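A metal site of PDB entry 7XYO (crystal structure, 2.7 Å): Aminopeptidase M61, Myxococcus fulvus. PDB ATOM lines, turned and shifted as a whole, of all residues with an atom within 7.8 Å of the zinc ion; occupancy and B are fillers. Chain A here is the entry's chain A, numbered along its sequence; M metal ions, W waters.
The side-chain carboxylate (OE1) of Glu 302 lies close to the side-chain hydroxyl (OH) of Tyr 366 (2.6 Å). The side-chain carboxylate (OE1) of Glu 306 is in hydrogen-bond range of a ring nitrogen (ND1) of His 273 (3.0 Å). A ring nitrogen (ND1) of His 277 lies within hydrogen-bond range of the backbone carbonyl oxygen (O) of Leu 280 (3.0 Å).
Residues that only touch the zinc ion: Tyr 366 (3.5 Å). Of the 11 residues printed, 4 come within 4 Å of the zinc ion. The nearest printed residue that does not touch the zinc ion is Glu 274 (4.3 Å).
The zinc ion is bound by the side-chain carboxylate of Glu 302 (2.0 Å), a ring nitrogen (NE2) of His 273 (2.3 Å) and a ring nitrogen (NE2) of His 277 (2.3 Å). Slightly farther from the zinc ion lies water W1 (2.7 Å).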
ATOM      1  N   HIS A 273     -10.700 -19.563  -0.674  1.00  0.00           N
ATOM      2  CA  HIS A 273      -9.264 -19.345  -0.881  1.00  0.00           C
ATOM      3  C   HIS A 273      -8.677 -18.470   0.212  1.00  0.00           C
ATOM      4  O   HIS A 273      -7.717 -18.860   0.898  1.00  0.00           O
ATOM      5  CB  HIS A 273      -9.027 -18.728  -2.266  1.00  0.00           C
ATOM      6  CG  HIS A 273      -7.578 -18.552  -2.606  1.00  0.00           C
ATOM      7  ND1 HIS A 273      -6.953 -19.279  -3.596  1.00  0.00           N
ATOM      8  CD2 HIS A 273      -6.637 -17.718  -2.088  1.00  0.00           C
ATOM      9  CE1 HIS A 273      -5.690 -18.910  -3.679  1.00  0.00           C
ATOM     10  NE2 HIS A 273      -5.470 -17.964  -2.779  1.00  0.00           N
ATOM     11  N   GLU A 274      -9.233 -17.272   0.400  1.00  0.00           N
ATOM     12  CA  GLU A 274      -8.634 -16.306   1.305  1.00  0.00           C
ATOM     13  C   GLU A 274      -8.685 -16.786   2.758  1.00  0.00           C
ATOM     14  O   GLU A 274      -7.730 -16.586   3.516  1.00  0.00           O
ATOM     15  CB  GLU A 274      -9.333 -14.949   1.173  1.00  0.00           C
ATOM     16  CG  GLU A 274      -9.133 -14.281  -0.173  1.00  0.00           C
ATOM     17  CD  GLU A 274      -7.695 -13.889  -0.447  1.00  0.00           C
ATOM     18  OE1 GLU A 274      -6.942 -13.657   0.532  1.00  0.00           O
ATOM     19  OE2 GLU A 274      -7.305 -13.810  -1.631  1.00  0.00           O
ATOM     20  N   HIS A 277      -5.945 -19.292   3.925  1.00  0.00           N
ATOM     21  CA  HIS A 277      -4.614 -18.806   4.253  1.00  0.00           C
ATOM     22  C   HIS A 277      -4.385 -18.687   5.749  1.00  0.00           C
ATOM     23  O   HIS A 277      -3.231 -18.547   6.177  1.00  0.00           O
ATOM     24  CB  HIS A 277      -4.359 -17.465   3.574  1.00  0.00           C
ATOM     25  CG  HIS A 277      -4.040 -17.590   2.115  1.00  0.00           C
ATOM     26  ND1 HIS A 277      -3.186 -18.545   1.620  1.00  0.00           N
ATOM     27  CD2 HIS A 277      -4.468 -16.870   1.048  1.00  0.00           C
ATOM     28  CE1 HIS A 277      -3.102 -18.419   0.303  1.00  0.00           C
ATOM     29  NE2 HIS A 277      -3.870 -17.414  -0.065  1.00  0.00           N
ATOM     30  N   LEU A 280      -3.119 -22.487   5.575  1.00  0.00           N
ATOM     31  CA  LEU A 280      -1.987 -22.692   4.691  1.00  0.00           C
ATOM     32  C   LEU A 280      -1.575 -21.380   3.966  1.00  0.00           C
ATOM     33  O   LEU A 280      -2.257 -20.965   3.096  1.00  0.00           O
ATOM     34  CB  LEU A 280      -2.268 -23.819   3.693  1.00  0.00           C
ATOM     35  CG  LEU A 280      -1.358 -23.960   2.463  1.00  0.00           C
ATOM     36  CD1 LEU A 280       0.098 -23.936   2.812  1.00  0.00           C
ATOM     37  CD2 LEU A 280      -1.639 -25.174   1.644  1.00  0.00           C
ATOM     38  N   PRO A 281      -0.446 -20.742   4.299  1.00  0.00           N
ATOM     39  CA  PRO A 281       0.737 -21.036   5.092  1.00  0.00           C
ATOM     40  C   PRO A 281       0.703 -20.506   6.482  1.00  0.00           C
ATOM     41  O   PRO A 281       1.670 -20.633   7.147  1.00  0.00           O
ATOM     42  CB  PRO A 281       1.827 -20.352   4.304  1.00  0.00           C
ATOM     43  CG  PRO A 281       1.181 -19.158   3.797  1.00  0.00           C
ATOM     44  CD  PRO A 281      -0.174 -19.610   3.429  1.00  0.00           C
ATOM     45  N   SER A 301       2.106 -22.498  -1.272  1.00  0.00           N
ATOM     46  CA  SER A 301       1.338 -21.597  -0.429  1.00  0.00           C
ATOM     47  C   SER A 301       0.243 -20.829  -1.129  1.00  0.00           C
ATOM     48  O   SER A 301      -0.711 -20.475  -0.515  1.00  0.00           O
ATOM     49  CB  SER A 301       2.229 -20.682   0.378  1.00  0.00           C
ATOM     50  OG  SER A 301       3.061 -19.928  -0.423  1.00  0.00           O
ATOM     51  N   GLU A 302       0.224 -20.760  -2.419  1.00  0.00           N
ATOM     52  CA  GLU A 302      -0.819 -20.167  -3.251  1.00  0.00           C
ATOM     53  C   GLU A 302      -1.475 -21.188  -4.166  1.00  0.00           C
ATOM     54  O   GLU A 302      -2.705 -21.260  -4.231  1.00  0.00           O
ATOM     55  CB  GLU A 302      -0.239 -19.020  -4.083  1.00  0.00           C
ATOM     56  CG  GLU A 302      -0.047 -17.706  -3.337  1.00  0.00           C
ATOM     57  CD  GLU A 302      -1.268 -17.307  -2.518  1.00  0.00           C
ATOM     58  OE1 GLU A 302      -2.378 -17.258  -3.087  1.00  0.00           O
ATOM     59  OE2 GLU A 302      -1.108 -17.042  -1.305  1.00  0.00           O
ATOM     60  N   GLY A 303      -0.679 -21.977  -4.891  1.00  0.00           N
ATOM     61  CA  GLY A 303      -1.244 -22.898  -5.869  1.00  0.00           C
ATOM     62  C   GLY A 303      -2.033 -24.023  -5.223  1.00  0.00           C
ATOM     63  O   GLY A 303      -3.164 -24.314  -5.622  1.00  0.00           O
ATOM     64  N   THR A 305      -3.290 -24.008  -2.257  1.00  0.00           N
ATOM     65  CA  THR A 305      -4.447 -23.427  -1.573  1.00  0.00           C
ATOM     66  C   THR A 305      -5.622 -23.262  -2.529  1.00  0.00           C
ATOM     67  O   THR A 305      -6.771 -23.521  -2.151  1.00  0.00           O
ATOM     68  CB  THR A 305      -4.064 -22.079  -0.958  1.00  0.00           C
ATOM     69  OG1 THR A 305      -3.028 -22.274   0.025  1.00  0.00           O
ATOM     70  CG2 THR A 305      -5.268 -21.432  -0.281  1.00  0.00           C
ATOM     71  N   GLU A 306      -5.347 -22.860  -3.765  1.00  0.00           N
ATOM     72  CA  GLU A 306      -6.406 -22.747  -4.756  1.00  0.00           C
ATOM     73  C   GLU A 306      -7.005 -24.116  -5.073  1.00  0.00           C
ATOM     74  O   GLU A 306      -8.229 -24.246  -5.251  1.00  0.00           O
ATOM     75  CB  GLU A 306      -5.864 -22.094  -6.033  1.00  0.00           C
ATOM     76  CG  GLU A 306      -6.827 -22.137  -7.218  1.00  0.00           C
ATOM     77  CD  GLU A 306      -8.026 -21.233  -7.034  1.00  0.00           C
ATOM     78  OE1 GLU A 306      -7.979 -20.333  -6.179  1.00  0.00           O
ATOM     79  OE2 GLU A 306      -9.033 -21.431  -7.749  1.00  0.00           O
ATOM     80  N   TYR A 366       0.452 -19.754  -9.259  1.00  0.00           N
ATOM     81  CA  TYR A 366      -0.923 -20.220  -9.059  1.00  0.00           C
ATOM     82  C   TYR A 366      -1.248 -21.363 -10.026  1.00  0.00           C
ATOM     83  O   TYR A 366      -1.740 -22.417  -9.607  1.00  0.00           O
ATOM     84  CB  TYR A 366      -1.906 -19.075  -9.243  1.00  0.00           C
ATOM     85  CG  TYR A 366      -1.983 -18.103  -8.093  1.00  0.00           C
ATOM     86  CD1 TYR A 366      -0.978 -17.169  -7.884  1.00  0.00           C
ATOM     87  CD2 TYR A 366      -3.052 -18.130  -7.199  1.00  0.00           C
ATOM     88  CE1 TYR A 366      -1.029 -16.281  -6.830  1.00  0.00           C
ATOM     89  CE2 TYR A 366      -3.116 -17.236  -6.144  1.00  0.00           C
ATOM     90  CZ  TYR A 366      -2.102 -16.314  -5.963  1.00  0.00           C
ATOM     91  OH  TYR A 366      -2.149 -15.417  -4.911  1.00  0.00           O
HETATM   92 ZN    ZN M   1      -3.948 -16.372  -2.121  1.00  0.00          ZN
HETATM   93  O   HOH W   1      -3.668 -13.684  -2.299  1.00  0.00           O
